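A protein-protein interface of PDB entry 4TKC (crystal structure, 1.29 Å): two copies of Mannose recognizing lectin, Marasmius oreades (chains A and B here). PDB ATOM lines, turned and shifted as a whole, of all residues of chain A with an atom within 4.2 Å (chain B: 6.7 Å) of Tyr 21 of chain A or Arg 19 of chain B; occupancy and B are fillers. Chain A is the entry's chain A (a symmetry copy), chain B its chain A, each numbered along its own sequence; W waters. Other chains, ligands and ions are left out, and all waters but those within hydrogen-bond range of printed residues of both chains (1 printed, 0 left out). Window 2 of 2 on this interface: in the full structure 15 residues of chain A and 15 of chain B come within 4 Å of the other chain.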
ATOM      1  N   TYR A   3     -26.377  19.755 -18.405  1.00  0.00           N
ATOM      2  CA  TYR A   3     -27.073  18.981 -17.419  1.00  0.00           C
ATOM      3  C   TYR A   3     -28.047  18.045 -18.073  1.00  0.00           C
ATOM      4  O   TYR A   3     -28.682  18.323 -19.088  1.00  0.00           O
ATOM      5  CB  TYR A   3     -27.869  19.916 -16.490  1.00  0.00           C
ATOM      6  CG  TYR A   3     -26.991  20.804 -15.653  1.00  0.00           C
ATOM      7  CD1 TYR A   3     -26.468  22.006 -16.152  1.00  0.00           C
ATOM      8  CD2 TYR A   3     -26.658  20.431 -14.372  1.00  0.00           C
ATOM      9  CE1 TYR A   3     -25.549  22.732 -15.408  1.00  0.00           C
ATOM     10  CE2 TYR A   3     -25.716  21.122 -13.644  1.00  0.00           C
ATOM     11  CZ  TYR A   3     -25.224  22.309 -14.127  1.00  0.00           C
ATOM     12  OH  TYR A   3     -24.267  22.970 -13.403  1.00  0.00           O
ATOM     13  N   VAL A   4     -28.008  16.817 -17.566  1.00  0.00           N
ATOM     14  CA  VAL A   4     -28.974  15.824 -17.988  1.00  0.00           C
ATOM     15  C   VAL A   4     -30.346  16.054 -17.299  1.00  0.00           C
ATOM     16  O   VAL A   4     -30.410  16.381 -16.128  1.00  0.00           O
ATOM     17  CB  VAL A   4     -28.418  14.410 -17.764  1.00  0.00           C
ATOM     18  CG1 VAL A   4     -29.473  13.385 -18.088  1.00  0.00           C
ATOM     19  CG2 VAL A   4     -27.187  14.209 -18.618  1.00  0.00           C
ATOM     20  N   PRO A   6     -33.610  14.105 -16.254  1.00  0.00           N
ATOM     21  CA  PRO A   6     -34.271  12.789 -16.144  1.00  0.00           C
ATOM     22  C   PRO A   6     -35.759  12.902 -15.902  1.00  0.00           C
ATOM     23  O   PRO A   6     -36.460  11.899 -15.845  1.00  0.00           O
ATOM     24  CB  PRO A   6     -33.611  12.159 -14.926  1.00  0.00           C
ATOM     25  CG  PRO A   6     -32.459  13.011 -14.554  1.00  0.00           C
ATOM     26  CD  PRO A   6     -32.755  14.382 -15.097  1.00  0.00           C
ATOM     27  N   ILE A  17     -32.707  14.847  -7.870  1.00  0.00           N
ATOM     28  CA  ILE A  17     -31.722  15.442  -8.788  1.00  0.00           C
ATOM     29  C   ILE A  17     -30.335  15.471  -8.166  1.00  0.00           C
ATOM     30  O   ILE A  17     -30.153  16.079  -7.110  1.00  0.00           O
ATOM     31  CB  ILE A  17     -31.968  16.954  -9.050  1.00  0.00           C
ATOM     32  CG1 ILE A  17     -33.420  17.295  -9.245  1.00  0.00           C
ATOM     33  CG2 ILE A  17     -31.122  17.430 -10.215  1.00  0.00           C
ATOM     34  CD1 ILE A  17     -33.636  18.780  -9.423  1.00  0.00           C
ATOM     35  N   GLY A  18     -29.364  14.757  -8.759  1.00  0.00           N
ATOM     36  CA  GLY A  18     -28.020  14.862  -8.271  1.00  0.00           C
ATOM     37  C   GLY A  18     -27.127  15.778  -9.089  1.00  0.00           C
ATOM     38  O   GLY A  18     -27.636  16.509  -9.956  1.00  0.00           O
ATOM     39  N   ARG A  19     -25.852  15.871  -8.737  1.00  0.00           N
ATOM     40  CA  ARG A  19     -24.887  16.762  -9.406  1.00  0.00           C
ATOM     41  C   ARG A  19     -24.759  16.422 -10.876  1.00  0.00           C
ATOM     42  O   ARG A  19     -24.596  15.220 -11.224  1.00  0.00           O
ATOM     43  CB  ARG A  19     -23.517  16.704  -8.755  1.00  0.00           C
ATOM     44  CG  ARG A  19     -23.517  17.131  -7.307  1.00  0.00           C
ATOM     45  CD  ARG A  19     -22.144  17.049  -6.670  1.00  0.00           C
ATOM     46  NE  ARG A  19     -22.158  17.621  -5.335  1.00  0.00           N
ATOM     47  CZ  ARG A  19     -21.110  17.657  -4.519  1.00  0.00           C
ATOM     48  NH1 ARG A  19     -21.202  18.210  -3.321  1.00  0.00           N
ATOM     49  NH2 ARG A  19     -19.942  17.205  -4.935  1.00  0.00           N
ATOM     50  N   GLY A  20     -24.913  17.453 -11.715  1.00  0.00           N
ATOM     51  CA  GLY A  20     -24.906  17.275 -13.156  1.00  0.00           C
ATOM     52  C   GLY A  20     -26.283  17.032 -13.789  1.00  0.00           C
ATOM     53  O   GLY A  20     -26.363  16.759 -14.988  1.00  0.00           O
ATOM     54  N   TYR A  21     -27.330  17.020 -12.956  1.00  0.00           N
ATOM     55  CA  TYR A  21     -28.691  16.813 -13.413  1.00  0.00           C
ATOM     56  C   TYR A  21     -29.498  18.083 -13.112  1.00  0.00           C
ATOM     57  O   TYR A  21     -29.126  18.852 -12.221  1.00  0.00           O
ATOM     58  CB  TYR A  21     -29.307  15.517 -12.799  1.00  0.00           C
ATOM     59  CG  TYR A  21     -28.497  14.271 -13.127  1.00  0.00           C
ATOM     60  CD1 TYR A  21     -27.297  14.076 -12.475  1.00  0.00           C
ATOM     61  CD2 TYR A  21     -28.741  13.542 -14.278  1.00  0.00           C
ATOM     62  CE1 TYR A  21     -26.488  12.995 -12.801  1.00  0.00           C
ATOM     63  CE2 TYR A  21     -27.945  12.430 -14.585  1.00  0.00           C
ATOM     64  CZ  TYR A  21     -26.781  12.249 -13.896  1.00  0.00           C
ATOM     65  OH  TYR A  21     -25.934  11.189 -14.204  1.00  0.00           O
ATOM     66  N   ALA A  22     -30.659  18.161 -13.741  1.00  0.00           N
ATOM     67  CA  ALA A  22     -31.489  19.396 -13.642  1.00  0.00           C
ATOM     68  C   ALA A  22     -32.918  19.128 -14.056  1.00  0.00           C
ATOM     69  O   ALA A  22     -33.167  18.223 -14.879  1.00  0.00           O
ATOM     70  CB  ALA A  22     -30.894  20.517 -14.483  1.00  0.00           C
ATOM     71  N   ARG A  33     -30.788  23.421 -11.449  1.00  0.00           N
ATOM     72  CA  ARG A  33     -29.592  22.580 -11.506  1.00  0.00           C
ATOM     73  C   ARG A  33     -29.062  22.252 -10.135  1.00  0.00           C
ATOM     74  O   ARG A  33     -29.024  23.106  -9.242  1.00  0.00           O
ATOM     75  CB  ARG A  33     -28.469  23.412 -12.158  1.00  0.00           C
ATOM     76  CG  ARG A  33     -28.751  23.998 -13.507  1.00  0.00           C
ATOM     77  CD  ARG A  33     -27.669  24.997 -13.902  1.00  0.00           C
ATOM     78  NE  ARG A  33     -27.978  25.522 -15.225  1.00  0.00           N
ATOM     79  CZ  ARG A  33     -27.287  26.450 -15.871  1.00  0.00           C
ATOM     80  NH1 ARG A  33     -26.254  27.064 -15.278  1.00  0.00           N
ATOM     81  NH2 ARG A  33     -27.673  26.787 -17.109  1.00  0.00           N
ATOM     82  N   VAL A  34     -28.482  21.047 -10.008  1.00  0.00           N
ATOM     83  CA  VAL A  34     -27.558  20.778  -8.914  1.00  0.00           C
ATOM     84  C   VAL A  34     -26.165  20.615  -9.547  1.00  0.00           C
ATOM     85  O   VAL A  34     -25.991  19.823 -10.491  1.00  0.00           O
ATOM     86  CB  VAL A  34     -27.958  19.515  -8.128  1.00  0.00           C
ATOM     87  CG1 VAL A  34     -26.943  19.193  -7.026  1.00  0.00           C
ATOM     88  CG2 VAL A  34     -29.340  19.682  -7.513  1.00  0.00           C
ATOM     89  N   TYR B   3     -20.014   6.504  -3.389  1.00  0.00           N
ATOM     90  CA  TYR B   3     -21.298   6.805  -3.954  1.00  0.00           C
ATOM     91  C   TYR B   3     -22.244   7.282  -2.891  1.00  0.00           C
ATOM     92  O   TYR B   3     -22.249   6.850  -1.740  1.00  0.00           O
ATOM     93  CB  TYR B   3     -21.898   5.536  -4.586  1.00  0.00           C
ATOM     94  CG  TYR B   3     -21.121   5.044  -5.775  1.00  0.00           C
ATOM     95  CD1 TYR B   3     -19.981   4.239  -5.630  1.00  0.00           C
ATOM     96  CD2 TYR B   3     -21.505   5.404  -7.046  1.00  0.00           C
ATOM     97  CE1 TYR B   3     -19.205   3.919  -6.735  1.00  0.00           C
ATOM     98  CE2 TYR B   3     -20.720   5.126  -8.140  1.00  0.00           C
ATOM     99  CZ  TYR B   3     -19.617   4.320  -7.997  1.00  0.00           C
ATOM    100  OH  TYR B   3     -18.831   4.076  -9.091  1.00  0.00           O
ATOM    101  N   VAL B  16     -34.657   8.037  -9.458  1.00  0.00           N
ATOM    102  CA  VAL B  16     -33.570   8.105 -10.394  1.00  0.00           C
ATOM    103  C   VAL B  16     -32.236   8.089  -9.683  1.00  0.00           C
ATOM    104  O   VAL B  16     -32.013   8.810  -8.707  1.00  0.00           O
ATOM    105  CB  VAL B  16     -33.613   9.412 -11.236  1.00  0.00           C
ATOM    106  CG1 VAL B  16     -32.301   9.580 -11.996  1.00  0.00           C
ATOM    107  CG2 VAL B  16     -34.765   9.332 -12.208  1.00  0.00           C
ATOM    108  N   ILE B  17     -31.362   7.184 -10.164  1.00  0.00           N
ATOM    109  CA  ILE B  17     -29.948   7.162  -9.757  1.00  0.00           C
ATOM    110  C   ILE B  17     -29.046   7.681 -10.865  1.00  0.00           C
ATOM    111  O   ILE B  17     -29.041   7.118 -11.962  1.00  0.00           O
ATOM    112  CB  ILE B  17     -29.391   5.725  -9.560  1.00  0.00           C
ATOM    113  CG1 ILE B  17     -30.350   4.807  -8.853  1.00  0.00           C
ATOM    114  CG2 ILE B  17     -28.046   5.773  -8.861  1.00  0.00           C
ATOM    115  CD1 ILE B  17     -29.813   3.399  -8.743  1.00  0.00           C
ATOM    116  N   GLY B  18     -28.337   8.797 -10.630  1.00  0.00           N
ATOM    117  CA  GLY B  18     -27.385   9.241 -11.605  1.00  0.00           C
ATOM    118  C   GLY B  18     -25.945   8.883 -11.284  1.00  0.00           C
ATOM    119  O   GLY B  18     -25.707   8.087 -10.359  1.00  0.00           O
ATOM    120  N   ARG B  19     -25.003   9.321 -12.108  1.00  0.00           N
ATOM    121  CA  ARG B  19     -23.572   9.003 -11.948  1.00  0.00           C
ATOM    122  C   ARG B  19     -23.048   9.499 -10.618  1.00  0.00           C
ATOM    123  O   ARG B  19     -23.303  10.678 -10.249  1.00  0.00           O
ATOM    124  CB  ARG B  19     -22.733   9.588 -13.069  1.00  0.00           C
ATOM    125  CG  ARG B  19     -23.106   9.073 -14.438  1.00  0.00           C
ATOM    126  CD  ARG B  19     -22.269   9.683 -15.545  1.00  0.00           C
ATOM    127  NE  ARG B  19     -22.548   9.041 -16.818  1.00  0.00           N
ATOM    128  CZ  ARG B  19     -21.994   9.388 -17.974  1.00  0.00           C
ATOM    129  NH1 ARG B  19     -22.290   8.742 -19.089  1.00  0.00           N
ATOM    130  NH2 ARG B  19     -21.079  10.338 -18.001  1.00  0.00           N
ATOM    131  N   GLY B  20     -22.403   8.585  -9.882  1.00  0.00           N
ATOM    132  CA  GLY B  20     -21.918   8.880  -8.546  1.00  0.00           C
ATOM    133  C   GLY B  20     -22.899   8.559  -7.411  1.00  0.00           C
ATOM    134  O   GLY B  20     -22.621   8.880  -6.254  1.00  0.00           O
ATOM    135  N   TYR B  21     -24.079   8.039  -7.770  1.00  0.00           N
ATOM    136  CA  TYR B  21     -25.101   7.676  -6.808  1.00  0.00           C
ATOM    137  C   TYR B  21     -25.322   6.159  -6.889  1.00  0.00           C
ATOM    138  O   TYR B  21     -25.030   5.550  -7.921  1.00  0.00           O
ATOM    139  CB  TYR B  21     -26.402   8.513  -7.014  1.00  0.00           C
ATOM    140  CG  TYR B  21     -26.156  10.012  -6.911  1.00  0.00           C
ATOM    141  CD1 TYR B  21     -25.515  10.647  -7.953  1.00  0.00           C
ATOM    142  CD2 TYR B  21     -26.228  10.665  -5.692  1.00  0.00           C
ATOM    143  CE1 TYR B  21     -25.201  11.997  -7.867  1.00  0.00           C
ATOM    144  CE2 TYR B  21     -25.943  12.036  -5.614  1.00  0.00           C
ATOM    145  CZ  TYR B  21     -25.340  12.640  -6.679  1.00  0.00           C
ATOM    146  OH  TYR B  21     -24.991  13.985  -6.626  1.00  0.00           O
ATOM    147  N   VAL B  34     -24.407   3.658 -10.404  1.00  0.00           N
ATOM    148  CA  VAL B  34     -24.193   4.199 -11.740  1.00  0.00           C
ATOM    149  C   VAL B  34     -22.886   5.008 -11.681  1.00  0.00           C
ATOM    150  O   VAL B  34     -22.724   5.880 -10.808  1.00  0.00           O
ATOM    151  CB  VAL B  34     -25.371   5.085 -12.191  1.00  0.00           C
ATOM    152  CG1 VAL B  34     -25.109   5.712 -13.564  1.00  0.00           C
ATOM    153  CG2 VAL B  34     -26.660   4.278 -12.237  1.00  0.00           C
ATOM    154  N   THR B  35     -21.903   4.598 -12.495  1.00  0.00           N
ATOM    155  CA  THR B  35     -20.531   5.095 -12.338  1.00  0.00           C
ATOM    156  C   THR B  35     -20.265   6.303 -13.209  1.00  0.00           C
ATOM    157  O   THR B  35     -20.951   6.521 -14.218  1.00  0.00           O
ATOM    158  CB  THR B  35     -19.461   4.002 -12.590  1.00  0.00           C
ATOM    159  OG1 THR B  35     -19.326   3.769 -13.987  1.00  0.00           O
ATOM    160  CG2 THR B  35     -19.827   2.679 -11.862  1.00  0.00           C
ATOM    161  N   ASP B  36     -19.228   7.053 -12.842  1.00  0.00           N
ATOM    162  CA  ASP B  36     -18.808   8.206 -13.661  1.00  0.00           C
ATOM    163  C   ASP B  36     -18.328   7.728 -15.036  1.00  0.00           C
ATOM    164  O   ASP B  36     -18.387   8.472 -15.998  1.00  0.00           O
ATOM    165  CB  ASP B  36     -17.698   9.009 -12.975  1.00  0.00           C
ATOM    166  CG  ASP B  36     -18.167   9.695 -11.682  1.00  0.00           C
ATOM    167  OD1 ASP B  36     -19.337  10.121 -11.616  1.00  0.00           O
ATOM    168  OD2 ASP B  36     -17.351   9.838 -10.749  1.00  0.00           O
ATOM    169  N   GLU B  37     -17.924   6.455 -15.121  1.00  0.00           N
ATOM    170  CA  GLU B  37     -17.516   5.842 -16.381  1.00  0.00           C
ATOM    171  C   GLU B  37     -18.754   5.392 -17.205  1.00  0.00           C
ATOM    172  O   GLU B  37     -18.608   4.854 -18.295  1.00  0.00           O
ATOM    173  CB  GLU B  37     -16.556   4.649 -16.122  1.00  0.00           C
ATOM    174  CG  GLU B  37     -15.215   5.032 -15.483  1.00  0.00           C
ATOM    175  CD  GLU B  37     -15.339   5.508 -14.028  1.00  0.00           C
ATOM    176  OE1 GLU B  37     -16.125   4.911 -13.254  1.00  0.00           O
ATOM    177  OE2 GLU B  37     -14.594   6.433 -13.629  1.00  0.00           O
ATOM    178  N   GLY B  38     -19.963   5.671 -16.703  1.00  0.00           N
ATOM    179  CA  GLY B  38     -21.200   5.306 -17.400  1.00  0.00           C
ATOM    180  C   GLY B  38     -21.531   3.822 -17.366  1.00  0.00           C
ATOM    181  O   GLY B  38     -22.277   3.313 -18.208  1.00  0.00           O
ATOM    182  N   ASN B  39     -21.072   3.155 -16.315  1.00  0.00           N
ATOM    183  CA  ASN B  39     -21.485   1.783 -16.134  1.00  0.00           C
ATOM    184  C   ASN B  39     -22.524   1.593 -15.040  1.00  0.00           C
ATOM    185  O   ASN B  39     -22.594   2.379 -14.097  1.00  0.00           O
ATOM    186  CB  ASN B  39     -20.279   0.870 -15.864  1.00  0.00           C
ATOM    187  CG  ASN B  39     -19.248   0.962 -16.967  1.00  0.00           C
ATOM    188  OD1 ASN B  39     -19.605   1.034 -18.137  1.00  0.00           O
ATOM    189  ND2 ASN B  39     -17.986   1.090 -16.603  1.00  0.00           N
ATOM    190  N   LYS B  56     -21.926   1.180 -22.103  1.00  0.00           N
ATOM    191  CA  LYS B  56     -23.000   1.907 -22.802  1.00  0.00           C
ATOM    192  C   LYS B  56     -23.220   3.384 -22.436  1.00  0.00           C
ATOM    193  O   LYS B  56     -24.174   3.988 -22.926  1.00  0.00           O
ATOM    194  CB  LYS B  56     -24.310   1.101 -22.681  1.00  0.00           C
ATOM    195  CG  LYS B  56     -24.129  -0.338 -23.161  1.00  0.00           C
ATOM    196  CD  LYS B  56     -25.441  -1.088 -23.330  1.00  0.00           C
ATOM    197  CE  LYS B  56     -26.256  -0.602 -24.520  1.00  0.00           C
ATOM    198  NZ  LYS B  56     -27.481  -1.419 -24.772  1.00  0.00           N
ATOM    199  N   ASN B  57     -22.287   3.978 -21.696  1.00  0.00           N
ATOM    200  CA  ASN B  57     -22.378   5.427 -21.385  1.00  0.00           C
ATOM    201  C   ASN B  57     -23.690   5.765 -20.680  1.00  0.00           C
ATOM    202  O   ASN B  57     -24.316   6.813 -20.958  1.00  0.00           O
ATOM    203  CB  ASN B  57     -22.200   6.284 -22.634  1.00  0.00           C
ATOM    204  CG  ASN B  57     -21.768   7.684 -22.300  1.00  0.00           C
ATOM    205  OD1 ASN B  57     -20.935   7.905 -21.413  1.00  0.00           O
ATOM    206  ND2 ASN B  57     -22.380   8.647 -22.971  1.00  0.00           N
ATOM    207  N   ALA B  58     -24.106   4.924 -19.733  1.00  0.00           N
ATOM    208  CA  ALA B  58     -25.276   5.216 -18.923  1.00  0.00           C
ATOM    209  C   ALA B  58     -25.099   6.517 -18.142  1.00  0.00           C
ATOM    210  O   ALA B  58     -24.027   6.765 -17.559  1.00  0.00           O
ATOM    211  CB  ALA B  58     -25.566   4.094 -17.968  1.00  0.00           C
ATOM    212  N   SER B  59     -26.146   7.361 -18.192  1.00  0.00           N
ATOM    213  CA  SER B  59     -26.227   8.554 -17.371  1.00  0.00           C
ATOM    214  C   SER B  59     -27.051   8.329 -16.096  1.00  0.00           C
ATOM    215  O   SER B  59     -26.759   8.895 -15.033  1.00  0.00           O
ATOM    216  CB  SER B  59     -26.850   9.658 -18.209  1.00  0.00           C
ATOM    217  OG  SER B  59     -26.989  10.873 -17.514  1.00  0.00           O
ATOM    218  N   PHE B  60     -28.129   7.570 -16.204  1.00  0.00           N
ATOM    219  CA  PHE B  60     -28.981   7.374 -15.041  1.00  0.00           C
ATOM    220  C   PHE B  60     -29.834   6.099 -15.220  1.00  0.00           C
ATOM    221  O   PHE B  60     -30.071   5.676 -16.345  1.00  0.00           O
ATOM    222  CB  PHE B  60     -29.839   8.653 -14.737  1.00  0.00           C
ATOM    223  CG  PHE B  60     -30.832   8.989 -15.804  1.00  0.00           C
ATOM    224  CD1 PHE B  60     -30.494   9.893 -16.802  1.00  0.00           C
ATOM    225  CD2 PHE B  60     -32.150   8.554 -15.727  1.00  0.00           C
ATOM    226  CE1 PHE B  60     -31.406  10.247 -17.770  1.00  0.00           C
ATOM    227  CE2 PHE B  60     -33.069   8.918 -16.708  1.00  0.00           C
ATOM    228  CZ  PHE B  60     -32.684   9.759 -17.732  1.00  0.00           C
ATOM    229  N   TYR B  72     -30.636   4.970 -19.012  1.00  0.00           N
ATOM    230  CA  TYR B  72     -30.589   5.906 -20.153  1.00  0.00           C
ATOM    231  C   TYR B  72     -29.212   6.513 -20.315  1.00  0.00           C
ATOM    232  O   TYR B  72     -28.540   6.797 -19.328  1.00  0.00           O
ATOM    233  CB  TYR B  72     -31.628   7.029 -19.996  1.00  0.00           C
ATOM    234  CG  TYR B  72     -33.071   6.615 -20.115  1.00  0.00           C
ATOM    235  CD1 TYR B  72     -33.674   6.499 -21.347  1.00  0.00           C
ATOM    236  CD2 TYR B  72     -33.859   6.360 -18.982  1.00  0.00           C
ATOM    237  CE1 TYR B  72     -34.991   6.097 -21.473  1.00  0.00           C
ATOM    238  CE2 TYR B  72     -35.181   5.974 -19.099  1.00  0.00           C
ATOM    239  CZ  TYR B  72     -35.762   5.868 -20.340  1.00  0.00           C
ATOM    240  OH  TYR B  72     -37.038   5.429 -20.482  1.00  0.00           O
ATOM    241  N   ASP B  73     -28.816   6.776 -21.554  1.00  0.00           N
ATOM    242  CA  ASP B  73     -27.594   7.561 -21.801  1.00  0.00           C
ATOM    243  C   ASP B  73     -27.945   9.089 -21.630  1.00  0.00           C
ATOM    244  O   ASP B  73     -29.110   9.447 -21.340  1.00  0.00           O
ATOM    245  CB  ASP B  73     -26.980   7.226 -23.175  1.00  0.00           C
ATOM    246  CG  ASP B  73     -27.537   8.096 -24.313  1.00  0.00           C
ATOM    247  OD1 ASP B  73     -28.724   8.470 -24.240  1.00  0.00           O
ATOM    248  OD2 ASP B  73     -26.795   8.282 -25.285  1.00  0.00           O
ATOM    249  N   PRO B  74     -26.950   9.989 -21.770  1.00  0.00           N
ATOM    250  CA  PRO B  74     -27.261  11.432 -21.547  1.00  0.00           C
ATOM    251  C   PRO B  74     -28.210  11.989 -22.581  1.00  0.00           C
ATOM    252  O   PRO B  74     -28.663  13.130 -22.396  1.00  0.00           O
ATOM    253  CB  PRO B  74     -25.898  12.114 -21.657  1.00  0.00           C
ATOM    254  CG  PRO B  74     -24.887  11.029 -21.440  1.00  0.00           C
ATOM    255  CD  PRO B  74     -25.507   9.781 -21.982  1.00  0.00           C
HETATM  256  O   HOH W   1     -23.041  13.167 -10.930  1.00  0.00           O
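Among the printed residues, merely in contact across the chains: Val 4 of chain A with Ser 59 of chain B (3.5 Å), Val 4 of chain A with Phe 60 of chain B (3.7 Å), Val 4 of chain A with Pro 74 of chain B (3.9 Å), Pro 6 of chain A with Phe 60 of chain B (3.7 Å), Gly 18 of chain A with Tyr 21 of chain B (3.6 Å) and Tyr 21 of chain A with Gly 18 of chain B (3.6 Å).
O of Tyr 21 of chain B lies within hydrogen-bond range of N of Val 34 of chain B (3.2 Å).
The backbone carbonyl oxygen (O) of Ala 58 of chain B lies within hydrogen-bond range of the guanidinium group (NE) of Arg 19 of chain B, 2.8 Å away.
O of Val 4 of chain A sits at hydrogen-bond distance from N of Ala 22 of chain A.
The backbone carbonyl oxygen of Gly 20 of chain A is in hydrogen-bond range of the backbone NH of Val 4 of chain A (3.1 Å).
O of Phe 60 of chain B lies within hydrogen-bond range of N of Tyr 72 of chain B.
O of Ser 59 of chain B sits at hydrogen-bond distance from N of Arg 19 of chain B, at 3.4 Å.
Of the printed residues of chain B, Val 4 of chain A touches Ser 59 (3.5 Å), Phe 60 (3.7 Å) and Pro 74 (3.9 Å).
Ile 17 of chain A touches none of the printed residues of chain B.
Of chain B, only Gly 18, Arg 19 and Ser 59 come within 4 Å of Tyr 21 of chain A.
Of the printed residues of chain A, Phe 60 of chain B touches Val 4 and Pro 6.
The nearest residue of chain B that does not touch Tyr 21 of chain A is Phe 60 of chain B (4.2 Å).
The nearest printed residue of chain A that does not touch Arg 19 of chain B is Arg 19 of chain A (4.8 Å).
The nearest printed residue of chain B that does not touch Gly 18 of chain A is Gly 18 of chain B (6.3 Å).
Water W1 lies within hydrogen-bond range of the backbone carbonyl oxygen of Arg 19 of chain A and the backbone carbonyl oxygen of Arg 19 of chain B.
Of the 11 printed residues of chain A, 5 touch a printed residue of chain B.
Printed residues of chain A that touch a printed residue of chain B: Val 4, Pro 6, Gly 18, Arg 19 and Tyr 21.
Hydrophobic or aromatic side chains of chain A that line the printed part of chain B: Val 4, Pro 6 and Tyr 21.
Among the printed residues, 9 pairs touch across the chains.
Gly 18 of chain A touches Tyr 21 of chain B, and with the chains exchanged Tyr 21 of chain A touches Gly 18 of chain B.
Arg 19 of chain A touches Tyr 21 of chain B, and with the chains exchanged Tyr 21 of chain A touches Arg 19 of chain B.
Positions printed for both chains: 3, 17, 18, 19, 20, 21 and 34.
N of Arg 19 of chain A sits at hydrogen-bond distance from OH of Tyr 21 of chain B.
OH of Tyr 21 of chain A is in hydrogen-bond range of N of Arg 19 of chain B (3.0 Å).
The backbone carbonyl oxygen (O) of Ser 59 of chain B is in hydrogen-bond range of the side-chain hydroxyl (OH) of Tyr 21 of chain A (2.6 Å).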
